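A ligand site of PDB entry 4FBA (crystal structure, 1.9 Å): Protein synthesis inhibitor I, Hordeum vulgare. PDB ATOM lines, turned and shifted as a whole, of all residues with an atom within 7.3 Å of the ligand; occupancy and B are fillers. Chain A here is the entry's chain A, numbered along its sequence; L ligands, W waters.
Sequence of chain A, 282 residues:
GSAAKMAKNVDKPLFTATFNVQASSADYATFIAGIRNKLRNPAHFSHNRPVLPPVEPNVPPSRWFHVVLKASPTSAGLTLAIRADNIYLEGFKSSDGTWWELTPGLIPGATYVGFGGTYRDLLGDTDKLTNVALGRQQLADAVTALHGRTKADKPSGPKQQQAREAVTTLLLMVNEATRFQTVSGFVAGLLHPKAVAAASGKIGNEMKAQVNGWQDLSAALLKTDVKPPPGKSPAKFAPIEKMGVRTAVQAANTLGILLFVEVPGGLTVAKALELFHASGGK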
ATOM      1  N   ILE A  82      10.800   2.553  -1.062  1.00  0.00           N
ATOM      2  CA  ILE A  82      10.356   1.824   0.121  1.00  0.00           C
ATOM      3  C   ILE A  82      11.467   0.903   0.601  1.00  0.00           C
ATOM      4  O   ILE A  82      12.137   0.248  -0.206  1.00  0.00           O
ATOM      5  CB  ILE A  82       9.082   1.002  -0.217  1.00  0.00           C
ATOM      6  CG1 ILE A  82       7.999   1.914  -0.816  1.00  0.00           C
ATOM      7  CG2 ILE A  82       8.564   0.283   1.006  1.00  0.00           C
ATOM      8  CD1 ILE A  82       6.729   1.169  -1.260  1.00  0.00           C
ATOM      9  N   ASN A  86      11.689  -3.520   6.035  1.00  0.00           N
ATOM     10  CA  ASN A  86      10.485  -3.348   6.846  1.00  0.00           C
ATOM     11  C   ASN A  86       9.325  -2.690   6.088  1.00  0.00           C
ATOM     12  O   ASN A  86       8.314  -2.321   6.694  1.00  0.00           O
ATOM     13  CB  ASN A  86      10.789  -2.564   8.126  1.00  0.00           C
ATOM     14  CG  ASN A  86      11.300  -1.173   7.850  1.00  0.00           C
ATOM     15  OD1 ASN A  86      11.339  -0.723   6.701  1.00  0.00           O
ATOM     16  ND2 ASN A  86      11.685  -0.455   8.913  1.00  0.00           N
ATOM     17  N   ILE A  87       9.487  -2.529   4.780  1.00  0.00           N
ATOM     18  CA  ILE A  87       8.458  -2.006   3.879  1.00  0.00           C
ATOM     19  C   ILE A  87       8.031  -0.583   4.259  1.00  0.00           C
ATOM     20  O   ILE A  87       6.866  -0.209   4.132  1.00  0.00           O
ATOM     21  CB  ILE A  87       7.236  -2.950   3.756  1.00  0.00           C
ATOM     22  CG1 ILE A  87       7.707  -4.404   3.691  1.00  0.00           C
ATOM     23  CG2 ILE A  87       6.426  -2.622   2.523  1.00  0.00           C
ATOM     24  CD1 ILE A  87       6.590  -5.425   3.713  1.00  0.00           C
ATOM     25  N   TYR A  88       8.978   0.217   4.730  1.00  0.00           N
ATOM     26  CA  TYR A  88       8.686   1.591   5.132  1.00  0.00           C
ATOM     27  C   TYR A  88       8.897   2.571   3.982  1.00  0.00           C
ATOM     28  O   TYR A  88       9.982   2.630   3.405  1.00  0.00           O
ATOM     29  CB  TYR A  88       9.542   1.999   6.334  1.00  0.00           C
ATOM     30  CG  TYR A  88       8.861   2.975   7.268  1.00  0.00           C
ATOM     31  CD1 TYR A  88       7.970   2.532   8.237  1.00  0.00           C
ATOM     32  CD2 TYR A  88       9.107   4.342   7.184  1.00  0.00           C
ATOM     33  CE1 TYR A  88       7.334   3.423   9.099  1.00  0.00           C
ATOM     34  CE2 TYR A  88       8.478   5.241   8.035  1.00  0.00           C
ATOM     35  CZ  TYR A  88       7.596   4.774   8.985  1.00  0.00           C
ATOM     36  OH  TYR A  88       6.979   5.661   9.835  1.00  0.00           O
ATOM     37  N   LEU A  89       7.846   3.321   3.646  1.00  0.00           N
ATOM     38  CA  LEU A  89       7.928   4.352   2.623  1.00  0.00           C
ATOM     39  C   LEU A  89       8.717   5.516   3.190  1.00  0.00           C
ATOM     40  O   LEU A  89       8.385   6.031   4.261  1.00  0.00           O
ATOM     41  CB  LEU A  89       6.515   4.828   2.256  1.00  0.00           C
ATOM     42  CG  LEU A  89       6.422   5.999   1.272  1.00  0.00           C
ATOM     43  CD1 LEU A  89       6.942   5.600  -0.101  1.00  0.00           C
ATOM     44  CD2 LEU A  89       4.977   6.510   1.192  1.00  0.00           C
ATOM     45  N   GLU A  90       9.777   5.940   2.498  1.00  0.00           N
ATOM     46  CA  GLU A  90      10.548   7.098   2.943  1.00  0.00           C
ATOM     47  C   GLU A  90      10.668   8.181   1.872  1.00  0.00           C
ATOM     48  O   GLU A  90      10.978   9.339   2.184  1.00  0.00           O
ATOM     49  CB  GLU A  90      11.942   6.683   3.419  1.00  0.00           C
ATOM     50  CG  GLU A  90      11.992   5.972   4.782  1.00  0.00           C
ATOM     51  CD  GLU A  90      11.710   6.901   5.961  1.00  0.00           C
ATOM     52  OE1 GLU A  90      11.392   8.084   5.740  1.00  0.00           O
ATOM     53  OE2 GLU A  90      11.827   6.434   7.118  1.00  0.00           O
ATOM     54  N   LEU A 102      10.469  11.732   3.527  1.00  0.00           N
ATOM     55  CA  LEU A 102       9.596  11.847   4.695  1.00  0.00           C
ATOM     56  C   LEU A 102      10.387  11.929   5.988  1.00  0.00           C
ATOM     57  O   LEU A 102       9.817  12.056   7.078  1.00  0.00           O
ATOM     58  CB  LEU A 102       8.607  10.673   4.753  1.00  0.00           C
ATOM     59  CG  LEU A 102       7.532  10.745   3.669  1.00  0.00           C
ATOM     60  CD1 LEU A 102       6.990   9.354   3.355  1.00  0.00           C
ATOM     61  CD2 LEU A 102       6.416  11.675   4.128  1.00  0.00           C
ATOM     62  N   GLY A 116       6.374  14.337   8.612  1.00  0.00           N
ATOM     63  CA  GLY A 116       6.973  13.027   8.829  1.00  0.00           C
ATOM     64  C   GLY A 116       6.161  11.889   8.238  1.00  0.00           C
ATOM     65  O   GLY A 116       5.038  12.086   7.770  1.00  0.00           O
ATOM     66  N   GLY A 117       6.721  10.677   8.295  1.00  0.00           N
ATOM     67  CA  GLY A 117       6.101   9.521   7.658  1.00  0.00           C
ATOM     68  C   GLY A 117       5.251   8.624   8.542  1.00  0.00           C
ATOM     69  O   GLY A 117       4.696   7.640   8.045  1.00  0.00           O
ATOM     70  N   THR A 118       5.125   8.938   9.825  1.00  0.00           N
ATOM     71  CA  THR A 118       4.312   8.108  10.734  1.00  0.00           C
ATOM     72  C   THR A 118       2.837   8.483  10.608  1.00  0.00           C
ATOM     73  O   THR A 118       2.516   9.574  10.156  1.00  0.00           O
ATOM     74  CB  THR A 118       4.764   8.247  12.203  1.00  0.00           C
ATOM     75  OG1 THR A 118       4.256   9.454  12.761  1.00  0.00           O
ATOM     76  CG2 THR A 118       6.280   8.248  12.290  1.00  0.00           C
ATOM     77  N   TYR A 119       1.938   7.589  11.013  1.00  0.00           N
ATOM     78  CA  TYR A 119       0.517   7.935  10.972  1.00  0.00           C
ATOM     79  C   TYR A 119       0.203   9.086  11.925  1.00  0.00           C
ATOM     80  O   TYR A 119      -0.652   9.923  11.619  1.00  0.00           O
ATOM     81  CB  TYR A 119      -0.351   6.707  11.270  1.00  0.00           C
ATOM     82  CG  TYR A 119      -0.388   5.688  10.141  1.00  0.00           C
ATOM     83  CD1 TYR A 119      -0.557   6.093   8.818  1.00  0.00           C
ATOM     84  CD2 TYR A 119      -0.248   4.340  10.402  1.00  0.00           C
ATOM     85  CE1 TYR A 119      -0.579   5.157   7.784  1.00  0.00           C
ATOM     86  CE2 TYR A 119      -0.267   3.398   9.376  1.00  0.00           C
ATOM     87  CZ  TYR A 119      -0.433   3.816   8.072  1.00  0.00           C
ATOM     88  OH  TYR A 119      -0.457   2.868   7.057  1.00  0.00           O
ATOM     89  N   ARG A 120       0.890   9.152  13.054  1.00  0.00           N
ATOM     90  CA  ARG A 120       0.775  10.312  13.936  1.00  0.00           C
ATOM     91  C   ARG A 120       1.102  11.599  13.163  1.00  0.00           C
ATOM     92  O   ARG A 120       0.375  12.594  13.248  1.00  0.00           O
ATOM     93  CB  ARG A 120       1.676  10.172  15.169  1.00  0.00           C
ATOM     94  CG  ARG A 120       1.602  11.366  16.129  1.00  0.00           C
ATOM     95  CD  ARG A 120       2.179  11.034  17.502  1.00  0.00           C
ATOM     96  NE  ARG A 120       3.518  11.594  17.713  1.00  0.00           N
ATOM     97  CZ  ARG A 120       4.234  11.425  18.822  1.00  0.00           C
ATOM     98  NH1 ARG A 120       3.739  10.705  19.820  1.00  0.00           N
ATOM     99  NH2 ARG A 120       5.439  11.961  18.939  1.00  0.00           N
ATOM    100  N   LEU A 122       1.004  11.979   9.843  1.00  0.00           N
ATOM    101  CA  LEU A 122       0.096  12.144   8.703  1.00  0.00           C
ATOM    102  C   LEU A 122      -1.351  12.438   9.107  1.00  0.00           C
ATOM    103  O   LEU A 122      -2.026  13.211   8.428  1.00  0.00           O
ATOM    104  CB  LEU A 122       0.134  10.898   7.828  1.00  0.00           C
ATOM    105  CG  LEU A 122       1.532  10.587   7.298  1.00  0.00           C
ATOM    106  CD1 LEU A 122       1.580   9.217   6.643  1.00  0.00           C
ATOM    107  CD2 LEU A 122       1.950  11.663   6.315  1.00  0.00           C
ATOM    108  N   THR A 126      -2.986   7.258  15.147  1.00  0.00           N
ATOM    109  CA  THR A 126      -3.161   5.959  14.473  1.00  0.00           C
ATOM    110  C   THR A 126      -4.589   5.419  14.591  1.00  0.00           C
ATOM    111  O   THR A 126      -4.868   4.317  14.111  1.00  0.00           O
ATOM    112  CB  THR A 126      -2.194   4.867  15.000  1.00  0.00           C
ATOM    113  OG1 THR A 126      -2.197   4.864  16.434  1.00  0.00           O
ATOM    114  CG2 THR A 126      -0.778   5.104  14.497  1.00  0.00           C
ATOM    115  N   LEU A 129      -7.065   5.961  11.169  1.00  0.00           N
ATOM    116  CA  LEU A 129      -6.902   5.045  10.026  1.00  0.00           C
ATOM    117  C   LEU A 129      -8.258   4.579   9.491  1.00  0.00           C
ATOM    118  O   LEU A 129      -8.419   4.383   8.285  1.00  0.00           O
ATOM    119  CB  LEU A 129      -6.055   3.833  10.406  1.00  0.00           C
ATOM    120  CG  LEU A 129      -4.535   3.979  10.430  1.00  0.00           C
ATOM    121  CD1 LEU A 129      -3.900   2.636  10.738  1.00  0.00           C
ATOM    122  CD2 LEU A 129      -4.039   4.537   9.106  1.00  0.00           C
ATOM    123  N   VAL A 167      -0.259  10.543   0.826  1.00  0.00           N
ATOM    124  CA  VAL A 167       0.687   9.583   1.369  1.00  0.00           C
ATOM    125  C   VAL A 167      -0.025   8.530   2.220  1.00  0.00           C
ATOM    126  O   VAL A 167       0.273   7.334   2.140  1.00  0.00           O
ATOM    127  CB  VAL A 167       1.826  10.284   2.171  1.00  0.00           C
ATOM    128  CG1 VAL A 167       2.671   9.257   2.919  1.00  0.00           C
ATOM    129  CG2 VAL A 167       2.702  11.106   1.254  1.00  0.00           C
ATOM    130  N   LEU A 171      -0.005   4.470   1.640  1.00  0.00           N
ATOM    131  CA  LEU A 171       0.484   3.574   2.691  1.00  0.00           C
ATOM    132  C   LEU A 171      -0.507   2.428   2.894  1.00  0.00           C
ATOM    133  O   LEU A 171      -0.109   1.269   2.980  1.00  0.00           O
ATOM    134  CB  LEU A 171       0.653   4.337   4.005  1.00  0.00           C
ATOM    135  CG  LEU A 171       1.892   5.222   4.109  1.00  0.00           C
ATOM    136  CD1 LEU A 171       1.989   5.841   5.506  1.00  0.00           C
ATOM    137  CD2 LEU A 171       3.147   4.425   3.796  1.00  0.00           C
ATOM    138  N   ASN A 175       1.570  -0.240   1.004  1.00  0.00           N
ATOM    139  CA  ASN A 175       2.419  -0.822   2.038  1.00  0.00           C
ATOM    140  C   ASN A 175       1.670  -1.771   2.970  1.00  0.00           C
ATOM    141  O   ASN A 175       2.130  -2.883   3.209  1.00  0.00           O
ATOM    142  CB  ASN A 175       3.157   0.271   2.835  1.00  0.00           C
ATOM    143  CG  ASN A 175       3.917   1.223   1.937  1.00  0.00           C
ATOM    144  OD1 ASN A 175       3.321   1.966   1.154  1.00  0.00           O
ATOM    145  ND2 ASN A 175       5.247   1.199   2.029  1.00  0.00           N
ATOM    146  N   GLU A 176       0.522  -1.337   3.489  1.00  0.00           N
ATOM    147  CA  GLU A 176      -0.232  -2.172   4.407  1.00  0.00           C
ATOM    148  C   GLU A 176      -0.881  -3.332   3.680  1.00  0.00           C
ATOM    149  O   GLU A 176      -1.021  -4.413   4.232  1.00  0.00           O
ATOM    150  CB  GLU A 176      -1.294  -1.355   5.162  1.00  0.00           C
ATOM    151  CG  GLU A 176      -0.758  -0.114   5.890  1.00  0.00           C
ATOM    152  CD  GLU A 176       0.234  -0.417   7.007  1.00  0.00           C
ATOM    153  OE1 GLU A 176       0.572  -1.604   7.254  1.00  0.00           O
ATOM    154  OE2 GLU A 176       0.688   0.545   7.674  1.00  0.00           O
ATOM    155  N   ARG A 179       1.645  -5.949   3.494  1.00  0.00           N
ATOM    156  CA  ARG A 179       1.844  -6.606   4.786  1.00  0.00           C
ATOM    157  C   ARG A 179       0.701  -7.555   5.166  1.00  0.00           C
ATOM    158  O   ARG A 179       0.928  -8.576   5.830  1.00  0.00           O
ATOM    159  CB  ARG A 179       2.002  -5.555   5.881  1.00  0.00           C
ATOM    160  CG  ARG A 179       3.329  -4.774   5.831  1.00  0.00           C
ATOM    161  CD  ARG A 179       3.228  -3.558   6.754  1.00  0.00           C
ATOM    162  NE  ARG A 179       4.501  -2.852   6.920  1.00  0.00           N
ATOM    163  CZ  ARG A 179       4.605  -1.530   7.062  1.00  0.00           C
ATOM    164  NH1 ARG A 179       3.512  -0.776   7.024  1.00  0.00           N
ATOM    165  NH2 ARG A 179       5.795  -0.960   7.219  1.00  0.00           N
ATOM    166  N   VAL A 211      -2.782  -3.507  11.434  1.00  0.00           N
ATOM    167  CA  VAL A 211      -1.832  -2.535  10.904  1.00  0.00           C
ATOM    168  C   VAL A 211      -0.963  -1.947  12.023  1.00  0.00           C
ATOM    169  O   VAL A 211       0.260  -1.807  11.887  1.00  0.00           O
ATOM    170  CB  VAL A 211      -2.565  -1.409  10.129  1.00  0.00           C
ATOM    171  CG1 VAL A 211      -1.678  -0.183   9.986  1.00  0.00           C
ATOM    172  CG2 VAL A 211      -3.030  -1.912   8.756  1.00  0.00           C
ATOM    173  N   ASN A 212      -1.598  -1.634  13.155  1.00  0.00           N
ATOM    174  CA  ASN A 212      -0.852  -1.070  14.276  1.00  0.00           C
ATOM    175  C   ASN A 212      -0.031  -2.073  15.100  1.00  0.00           C
ATOM    176  O   ASN A 212       0.714  -1.686  16.012  1.00  0.00           O
ATOM    177  CB  ASN A 212      -1.782  -0.240  15.182  1.00  0.00           C
ATOM    178  CG  ASN A 212      -2.224   1.061  14.523  1.00  0.00           C
ATOM    179  OD1 ASN A 212      -1.467   1.684  13.776  1.00  0.00           O
ATOM    180  ND2 ASN A 212      -3.465   1.475  14.808  1.00  0.00           N
ATOM    181  N   TRP A 214       1.691  -4.999  13.474  1.00  0.00           N
ATOM    182  CA  TRP A 214       2.367  -5.869  12.520  1.00  0.00           C
ATOM    183  C   TRP A 214       3.506  -6.676  13.158  1.00  0.00           C
ATOM    184  O   TRP A 214       3.612  -7.883  12.943  1.00  0.00           O
ATOM    185  CB  TRP A 214       2.891  -5.050  11.344  1.00  0.00           C
ATOM    186  CG  TRP A 214       3.543  -5.846  10.232  1.00  0.00           C
ATOM    187  CD1 TRP A 214       3.122  -7.052   9.713  1.00  0.00           C
ATOM    188  CD2 TRP A 214       4.722  -5.505   9.523  1.00  0.00           C
ATOM    189  NE1 TRP A 214       3.975  -7.454   8.704  1.00  0.00           N
ATOM    190  CE2 TRP A 214       4.967  -6.517   8.573  1.00  0.00           C
ATOM    191  CE3 TRP A 214       5.593  -4.414   9.580  1.00  0.00           C
ATOM    192  CZ2 TRP A 214       6.059  -6.466   7.687  1.00  0.00           C
ATOM    193  CZ3 TRP A 214       6.670  -4.371   8.707  1.00  0.00           C
ATOM    194  CH2 TRP A 214       6.891  -5.394   7.774  1.00  0.00           C
HETATM  195  N1  LIG L   1       3.150   3.057   8.813  1.00  0.00           N
HETATM  196  C1  LIG L   1       3.158   4.369   9.180  1.00  0.00           C
HETATM  197  N2  LIG L   1       3.960   5.113   8.449  1.00  0.00           N
HETATM  198  C2  LIG L   1       4.494   4.240   7.519  1.00  0.00           C
HETATM  199  C3  LIG L   1       5.423   4.408   6.463  1.00  0.00           C
HETATM  200  N3  LIG L   1       5.981   5.585   6.135  1.00  0.00           N
HETATM  201  N4  LIG L   1       5.738   3.311   5.744  1.00  0.00           N
HETATM  202  C4  LIG L   1       5.186   2.141   6.062  1.00  0.00           C
HETATM  203  N5  LIG L   1       4.317   1.861   7.034  1.00  0.00           N
HETATM  204  C5  LIG L   1       4.017   2.966   7.739  1.00  0.00           C
HETATM  205  O   HOH W   1       2.089   0.832  10.079  1.00  0.00           O
HETATM  206  O   HOH W   2       2.962   5.175  12.484  1.00  0.00           O
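The guanidinium group of Arg 179 sits at hydrogen-bond distance from the backbone carbonyl oxygen of Ile 87 (3.4 Å).
The guanidinium group of Arg 179 lies within salt-bridge range of the side-chain carboxylate of Glu 176, at 3.1 Å.
The guanidinium group (NH2) of Arg 179 lies within hydrogen-bond range of the backbone carbonyl oxygen (O) of Asn 86 (2.9 Å).
The backbone NH of Tyr 88 lies within hydrogen-bond range of the side-chain amide oxygen of Asn 86 (3.2 Å).
N of Glu 176 sits at hydrogen-bond distance from O of Leu 171 (2.7 Å).
The backbone carbonyl oxygen of Ile 87 sits at hydrogen-bond distance from the side-chain amide nitrogen of Asn 175.
OH of Tyr 119 sits at hydrogen-bond distance from OE2 of Glu 176 (2.7 Å).
The side-chain hydroxyl (OG1) of Thr 118 lies close to the backbone NH (N) of Arg 120 (3.4 Å).
Merely in contact with the ligand: Leu 171 (3.4 Å), Ile 87 (3.5 Å), Tyr 119 (3.5 Å), Glu 176 (3.7 Å) and Thr 118 (3.8 Å).
Hydrophobic or aromatic side chains within 4 Å of the ligand: Tyr 88, Leu 89, Tyr 119 and Leu 171.
Within 4 Å of the ligand: Ile 87, Tyr 88, Leu 89, Gly 117, Thr 118, Tyr 119, Leu 171, Glu 176 and Arg 179.
Water W1 bridges N1 of the ligand (2.8 Å) and OE2 of Glu 176 (2.8 Å).
N3 of the ligand lies within hydrogen-bond range of O of Gly 117 (3.1 Å).
NH1 of Arg 179 sits at hydrogen-bond distance from N5 of the ligand (2.8 Å).
The backbone NH (N) of Leu 89 is in hydrogen-bond range of a nitrogen (N4) of the ligand (3.0 Å).
The backbone carbonyl oxygen (O) of Leu 89 sits at hydrogen-bond distance from a nitrogen (N3) of the ligand (3.1 Å).
OH of Tyr 88 sits at hydrogen-bond distance from N2 of the ligand (3.4 Å).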
